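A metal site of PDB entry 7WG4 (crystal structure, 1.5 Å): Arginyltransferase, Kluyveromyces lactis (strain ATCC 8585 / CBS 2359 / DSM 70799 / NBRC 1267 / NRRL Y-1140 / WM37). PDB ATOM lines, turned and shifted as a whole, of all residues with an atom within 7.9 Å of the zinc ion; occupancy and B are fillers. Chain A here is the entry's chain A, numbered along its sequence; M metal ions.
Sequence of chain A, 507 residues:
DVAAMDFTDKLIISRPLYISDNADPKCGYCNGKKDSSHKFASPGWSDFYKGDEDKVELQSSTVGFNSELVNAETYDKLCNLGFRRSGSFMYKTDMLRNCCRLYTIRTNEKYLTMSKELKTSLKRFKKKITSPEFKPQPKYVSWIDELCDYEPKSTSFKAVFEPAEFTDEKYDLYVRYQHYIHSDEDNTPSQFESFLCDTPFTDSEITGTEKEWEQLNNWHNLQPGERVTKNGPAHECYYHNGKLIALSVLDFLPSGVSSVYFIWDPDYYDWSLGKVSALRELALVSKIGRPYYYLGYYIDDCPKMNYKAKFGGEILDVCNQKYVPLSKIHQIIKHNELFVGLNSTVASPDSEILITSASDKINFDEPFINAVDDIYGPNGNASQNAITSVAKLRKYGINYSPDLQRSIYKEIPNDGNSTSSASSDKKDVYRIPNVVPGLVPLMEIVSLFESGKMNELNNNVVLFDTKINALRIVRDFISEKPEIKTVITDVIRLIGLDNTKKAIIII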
ATOM      1  N   ALA A  23     -32.713  -2.193 -16.788  1.00  0.00           N
ATOM      2  CA  ALA A  23     -31.477  -2.658 -16.206  1.00  0.00           C
ATOM      3  C   ALA A  23     -31.613  -2.820 -14.685  1.00  0.00           C
ATOM      4  O   ALA A  23     -30.844  -3.549 -14.089  1.00  0.00           O
ATOM      5  CB  ALA A  23     -30.328  -1.718 -16.554  1.00  0.00           C
ATOM      6  N   ASP A  24     -32.481  -2.000 -14.063  1.00  0.00           N
ATOM      7  CA  ASP A  24     -32.913  -2.206 -12.697  1.00  0.00           C
ATOM      8  C   ASP A  24     -34.157  -3.072 -12.764  1.00  0.00           C
ATOM      9  O   ASP A  24     -35.233  -2.591 -13.149  1.00  0.00           O
ATOM     10  CB  ASP A  24     -33.214  -0.876 -12.011  1.00  0.00           C
ATOM     11  CG  ASP A  24     -33.551  -1.074 -10.533  1.00  0.00           C
ATOM     12  OD1 ASP A  24     -33.706  -2.250 -10.109  1.00  0.00           O
ATOM     13  OD2 ASP A  24     -33.599  -0.059  -9.826  1.00  0.00           O
ATOM     14  N   LYS A  26     -32.521  -6.074 -14.050  1.00  0.00           N
ATOM     15  CA  LYS A  26     -32.008  -7.163 -14.907  1.00  0.00           C
ATOM     16  C   LYS A  26     -30.487  -7.195 -14.994  1.00  0.00           C
ATOM     17  O   LYS A  26     -29.917  -8.278 -15.102  1.00  0.00           O
ATOM     18  CB  LYS A  26     -32.636  -7.077 -16.275  1.00  0.00           C
ATOM     19  CG  LYS A  26     -31.927  -7.909 -17.369  1.00  0.00           C
ATOM     20  CD  LYS A  26     -32.590  -7.772 -18.725  1.00  0.00           C
ATOM     21  CE  LYS A  26     -31.932  -8.708 -19.759  1.00  0.00           C
ATOM     22  NZ  LYS A  26     -32.294  -8.356 -21.148  1.00  0.00           N
ATOM     23  N   CYS A  27     -29.785  -6.059 -14.961  1.00  0.00           N
ATOM     24  CA  CYS A  27     -28.325  -6.093 -15.083  1.00  0.00           C
ATOM     25  C   CYS A  27     -27.705  -6.422 -13.742  1.00  0.00           C
ATOM     26  O   CYS A  27     -27.775  -5.621 -12.791  1.00  0.00           O
ATOM     27  CB  CYS A  27     -27.685  -4.762 -15.592  1.00  0.00           C
ATOM     28  SG  CYS A  27     -25.971  -4.844 -15.773  1.00  0.00           S
ATOM     29  N   GLY A  28     -26.994  -7.521 -13.686  1.00  0.00           N
ATOM     30  CA  GLY A  28     -26.299  -7.838 -12.434  1.00  0.00           C
ATOM     31  C   GLY A  28     -25.001  -7.147 -12.237  1.00  0.00           C
ATOM     32  O   GLY A  28     -24.409  -7.225 -11.149  1.00  0.00           O
ATOM     33  N   TYR A  29     -24.519  -6.389 -13.237  1.00  0.00           N
ATOM     34  CA  TYR A  29     -23.298  -5.677 -13.058  1.00  0.00           C
ATOM     35  C   TYR A  29     -23.522  -4.299 -12.456  1.00  0.00           C
ATOM     36  O   TYR A  29     -22.736  -3.880 -11.608  1.00  0.00           O
ATOM     37  CB  TYR A  29     -22.577  -5.501 -14.392  1.00  0.00           C
ATOM     38  CG  TYR A  29     -22.397  -6.798 -15.160  1.00  0.00           C
ATOM     39  CD1 TYR A  29     -21.589  -7.809 -14.694  1.00  0.00           C
ATOM     40  CD2 TYR A  29     -23.042  -6.971 -16.384  1.00  0.00           C
ATOM     41  CE1 TYR A  29     -21.442  -8.970 -15.436  1.00  0.00           C
ATOM     42  CE2 TYR A  29     -22.882  -8.105 -17.103  1.00  0.00           C
ATOM     43  CZ  TYR A  29     -22.117  -9.072 -16.635  1.00  0.00           C
ATOM     44  OH  TYR A  29     -22.020 -10.201 -17.478  1.00  0.00           O
ATOM     45  N   CYS A  30     -24.565  -3.590 -12.870  1.00  0.00           N
ATOM     46  CA  CYS A  30     -24.763  -2.223 -12.395  1.00  0.00           C
ATOM     47  C   CYS A  30     -26.076  -2.065 -11.660  1.00  0.00           C
ATOM     48  O   CYS A  30     -26.286  -1.025 -11.021  1.00  0.00           O
ATOM     49  CB  CYS A  30     -24.695  -1.182 -13.564  1.00  0.00           C
ATOM     50  SG  CYS A  30     -26.119  -1.191 -14.698  1.00  0.00           S
ATOM     51  N   ASN A  31     -26.983  -2.993 -11.768  1.00  0.00           N
ATOM     52  CA  ASN A  31     -28.314  -2.921 -11.217  1.00  0.00           C
ATOM     53  C   ASN A  31     -29.081  -1.704 -11.666  1.00  0.00           C
ATOM     54  O   ASN A  31     -30.023  -1.244 -10.989  1.00  0.00           O
ATOM     55  CB  ASN A  31     -28.229  -2.964  -9.664  1.00  0.00           C
ATOM     56  CG  ASN A  31     -27.257  -4.038  -9.167  1.00  0.00           C
ATOM     57  OD1 ASN A  31     -27.557  -5.231  -9.299  1.00  0.00           O
ATOM     58  ND2 ASN A  31     -26.085  -3.630  -8.572  1.00  0.00           N
ATOM     59  N   GLY A  32     -28.711  -1.153 -12.816  1.00  0.00           N
ATOM     60  CA  GLY A  32     -29.375   0.005 -13.338  1.00  0.00           C
ATOM     61  C   GLY A  32     -28.970   1.308 -12.671  1.00  0.00           C
ATOM     62  O   GLY A  32     -29.595   2.336 -13.003  1.00  0.00           O
ATOM     63  N   LYS A  33     -27.865   1.319 -11.937  1.00  0.00           N
ATOM     64  CA  LYS A  33     -27.388   2.500 -11.176  1.00  0.00           C
ATOM     65  C   LYS A  33     -26.111   3.022 -11.768  1.00  0.00           C
ATOM     66  O   LYS A  33     -25.016   2.452 -11.563  1.00  0.00           O
ATOM     67  CB  LYS A  33     -27.166   2.184  -9.692  1.00  0.00           C
ATOM     68  CG  LYS A  33     -28.333   1.534  -8.991  1.00  0.00           C
ATOM     69  CD  LYS A  33     -29.667   2.152  -9.281  1.00  0.00           C
ATOM     70  CE  LYS A  33     -30.818   1.436  -8.521  1.00  0.00           C
ATOM     71  NZ  LYS A  33     -30.577  -0.048  -8.295  1.00  0.00           N
ATOM     72  N   LYS A  34     -26.194   4.181 -12.452  1.00  0.00           N
ATOM     73  CA  LYS A  34     -25.059   4.858 -13.003  1.00  0.00           C
ATOM     74  C   LYS A  34     -25.115   6.367 -12.686  1.00  0.00           C
ATOM     75  O   LYS A  34     -26.229   6.896 -12.630  1.00  0.00           O
ATOM     76  CB  LYS A  34     -25.017   4.704 -14.531  1.00  0.00           C
ATOM     77  CG  LYS A  34     -24.977   3.243 -15.012  1.00  0.00           C
ATOM     78  CD  LYS A  34     -23.565   2.852 -15.245  1.00  0.00           C
ATOM     79  CE  LYS A  34     -23.446   1.479 -15.875  1.00  0.00           C
ATOM     80  NZ  LYS A  34     -22.256   0.839 -15.325  1.00  0.00           N
ATOM     81  N   LEU A  58     -32.419   3.216 -18.099  1.00  0.00           N
ATOM     82  CA  LEU A  58     -31.413   2.315 -18.680  1.00  0.00           C
ATOM     83  C   LEU A  58     -31.991   0.922 -18.891  1.00  0.00           C
ATOM     84  O   LEU A  58     -32.715   0.382 -18.042  1.00  0.00           O
ATOM     85  CB  LEU A  58     -30.222   2.223 -17.738  1.00  0.00           C
ATOM     86  CG  LEU A  58     -29.318   3.461 -17.754  1.00  0.00           C
ATOM     87  CD1 LEU A  58     -28.206   3.251 -16.780  1.00  0.00           C
ATOM     88  CD2 LEU A  58     -28.799   3.841 -19.133  1.00  0.00           C
ATOM     89  N   GLN A  59     -31.654   0.323 -20.036  1.00  0.00           N
ATOM     90  CA  GLN A  59     -32.050  -1.034 -20.386  1.00  0.00           C
ATOM     91  C   GLN A  59     -30.849  -1.941 -20.451  1.00  0.00           C
ATOM     92  O   GLN A  59     -29.729  -1.499 -20.711  1.00  0.00           O
ATOM     93  CB  GLN A  59     -32.741  -1.088 -21.749  1.00  0.00           C
ATOM     94  CG  GLN A  59     -33.901  -0.110 -21.892  1.00  0.00           C
ATOM     95  CD  GLN A  59     -35.050  -0.486 -20.996  1.00  0.00           C
ATOM     96  OE1 GLN A  59     -35.747  -1.473 -21.261  1.00  0.00           O
ATOM     97  NE2 GLN A  59     -35.299   0.319 -19.961  1.00  0.00           N
ATOM     98  N   SER A  60     -31.086  -3.245 -20.191  1.00  0.00           N
ATOM     99  CA  SER A  60     -30.110  -4.313 -20.386  1.00  0.00           C
ATOM    100  C   SER A  60     -30.639  -5.139 -21.554  1.00  0.00           C
ATOM    101  O   SER A  60     -31.783  -5.534 -21.539  1.00  0.00           O
ATOM    102  CB  SER A  60     -29.941  -5.112 -19.126  1.00  0.00           C
ATOM    103  OG  SER A  60     -28.920  -6.121 -19.206  1.00  0.00           O
ATOM    104  N   ASN A  98     -27.011  -1.026 -24.332  1.00  0.00           N
ATOM    105  CA  ASN A  98     -26.891  -1.667 -23.020  1.00  0.00           C
ATOM    106  C   ASN A  98     -26.417  -0.654 -21.969  1.00  0.00           C
ATOM    107  O   ASN A  98     -25.638   0.258 -22.246  1.00  0.00           O
ATOM    108  CB  ASN A  98     -25.914  -2.833 -23.069  1.00  0.00           C
ATOM    109  CG  ASN A  98     -26.141  -3.817 -21.891  1.00  0.00           C
ATOM    110  OD1 ASN A  98     -27.220  -4.336 -21.700  1.00  0.00           O
ATOM    111  ND2 ASN A  98     -25.117  -4.044 -21.185  1.00  0.00           N
ATOM    112  N   CYS A  99     -26.901  -0.849 -20.748  1.00  0.00           N
ATOM    113  CA  CYS A  99     -26.455  -0.020 -19.621  1.00  0.00           C
ATOM    114  C   CYS A  99     -24.942  -0.026 -19.449  1.00  0.00           C
ATOM    115  O   CYS A  99     -24.319   1.033 -19.245  1.00  0.00           O
ATOM    116  CB  CYS A  99     -27.143  -0.529 -18.343  1.00  0.00           C
ATOM    117  SG  CYS A  99     -27.012  -2.341 -18.156  1.00  0.00           S
ATOM    118  N   CYS A 100     -24.316  -1.203 -19.507  1.00  0.00           N
ATOM    119  CA  CYS A 100     -22.916  -1.428 -19.295  1.00  0.00           C
ATOM    120  C   CYS A 100     -22.212  -1.804 -20.592  1.00  0.00           C
ATOM    121  O   CYS A 100     -22.805  -2.503 -21.467  1.00  0.00           O
ATOM    122  CB  CYS A 100     -22.701  -2.578 -18.351  1.00  0.00           C
ATOM    123  SG  CYS A 100     -23.162  -2.199 -16.624  1.00  0.00           S
ATOM    124  N   ARG A 101     -21.051  -1.222 -20.794  1.00  0.00           N
ATOM    125  CA  ARG A 101     -20.220  -1.515 -21.971  1.00  0.00           C
ATOM    126  C   ARG A 101     -19.335  -2.731 -21.721  1.00  0.00           C
ATOM    127  O   ARG A 101     -18.402  -2.695 -20.931  1.00  0.00           O
ATOM    128  CB  ARG A 101     -19.392  -0.283 -22.336  1.00  0.00           C
ATOM    129  CG  ARG A 101     -19.302  -0.070 -23.894  1.00  0.00           C
ATOM    130  CD  ARG A 101     -20.627   0.310 -24.478  1.00  0.00           C
ATOM    131  NE  ARG A 101     -21.116   1.522 -23.850  1.00  0.00           N
ATOM    132  CZ  ARG A 101     -22.348   1.676 -23.400  1.00  0.00           C
ATOM    133  NH1 ARG A 101     -23.319   0.863 -23.758  1.00  0.00           N
ATOM    134  NH2 ARG A 101     -22.610   2.585 -22.470  1.00  0.00           N
ATOM    135  N   LEU A 102     -19.640  -3.831 -22.429  1.00  0.00           N
ATOM    136  CA  LEU A 102     -18.962  -5.113 -22.265  1.00  0.00           C
ATOM    137  C   LEU A 102     -18.059  -5.283 -23.462  1.00  0.00           C
ATOM    138  O   LEU A 102     -18.542  -5.207 -24.615  1.00  0.00           O
ATOM    139  CB  LEU A 102     -19.947  -6.272 -22.145  1.00  0.00           C
ATOM    140  CG  LEU A 102     -20.547  -6.515 -20.785  1.00  0.00           C
ATOM    141  CD1 LEU A 102     -21.467  -5.431 -20.349  1.00  0.00           C
ATOM    142  CD2 LEU A 102     -21.287  -7.850 -20.794  1.00  0.00           C
ATOM    143  N   ILE A 299     -15.611  -5.042 -18.205  1.00  0.00           N
ATOM    144  CA  ILE A 299     -16.424  -3.834 -18.017  1.00  0.00           C
ATOM    145  C   ILE A 299     -15.543  -2.886 -17.179  1.00  0.00           C
ATOM    146  O   ILE A 299     -15.241  -3.227 -16.025  1.00  0.00           O
ATOM    147  CB  ILE A 299     -17.756  -4.095 -17.346  1.00  0.00           C
ATOM    148  CG1 ILE A 299     -18.573  -5.176 -18.040  1.00  0.00           C
ATOM    149  CG2 ILE A 299     -18.515  -2.805 -17.294  1.00  0.00           C
ATOM    150  CD1 ILE A 299     -19.824  -5.556 -17.244  1.00  0.00           C
ATOM    151  N   ASP A 301     -15.970  -0.070 -15.600  1.00  0.00           N
ATOM    152  CA  ASP A 301     -16.493   0.462 -14.341  1.00  0.00           C
ATOM    153  C   ASP A 301     -17.081  -0.575 -13.404  1.00  0.00           C
ATOM    154  O   ASP A 301     -17.759  -0.195 -12.436  1.00  0.00           O
ATOM    155  CB  ASP A 301     -17.501   1.589 -14.673  1.00  0.00           C
ATOM    156  CG  ASP A 301     -18.870   1.116 -15.101  1.00  0.00           C
ATOM    157  OD1 ASP A 301     -19.076  -0.117 -15.302  1.00  0.00           O
ATOM    158  OD2 ASP A 301     -19.797   2.014 -15.346  1.00  0.00           O
ATOM    159  N   ASN A 336     -17.429   4.351 -19.333  1.00  0.00           N
ATOM    160  CA  ASN A 336     -18.423   3.430 -19.878  1.00  0.00           C
ATOM    161  C   ASN A 336     -18.773   3.702 -21.342  1.00  0.00           C
ATOM    162  O   ASN A 336     -19.856   3.317 -21.791  1.00  0.00           O
ATOM    163  CB  ASN A 336     -19.671   3.453 -18.988  1.00  0.00           C
ATOM    164  CG  ASN A 336     -20.620   2.227 -19.200  1.00  0.00           C
ATOM    165  OD1 ASN A 336     -20.139   1.084 -19.286  1.00  0.00           O
ATOM    166  ND2 ASN A 336     -21.898   2.483 -19.208  1.00  0.00           N
HETATM  167 ZN    ZN M   1     -25.527  -2.608 -16.391  1.00  0.00          ZN
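SG of Cys 100 sits close to NZ of Lys 34.
The backbone carbonyl oxygen (O) of Cys 100 is in hydrogen-bond range of the side-chain amide nitrogen (ND2) of Asn 98, 2.8 Å away.
N of Gly 32 sits close to SG of Cys 30, 3.2 Å away.
The backbone carbonyl oxygen of Cys 99 lies within hydrogen-bond range of the side-chain amide nitrogen of Asn 336 (2.8 Å).
SG of Cys 27 sits close to N of Tyr 29.
N of Cys 99 lies within hydrogen-bond range of O of Gln 59 (2.9 Å).
Of the 22 residues printed, 4 come within 4 Å of the zinc ion.
Along chain A the residues within 4 Å of the zinc ion span positions 27 to 100.
The zinc ion is bound by the side-chain sulfur of Cys 30 (2.3 Å), the side-chain sulfur of Cys 99 (2.3 Å), the side-chain sulfur of Cys 27 (2.4 Å) and the side-chain sulfur of Cys 100 (2.4 Å).
The zinc ion has four donor atoms within binding distance.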
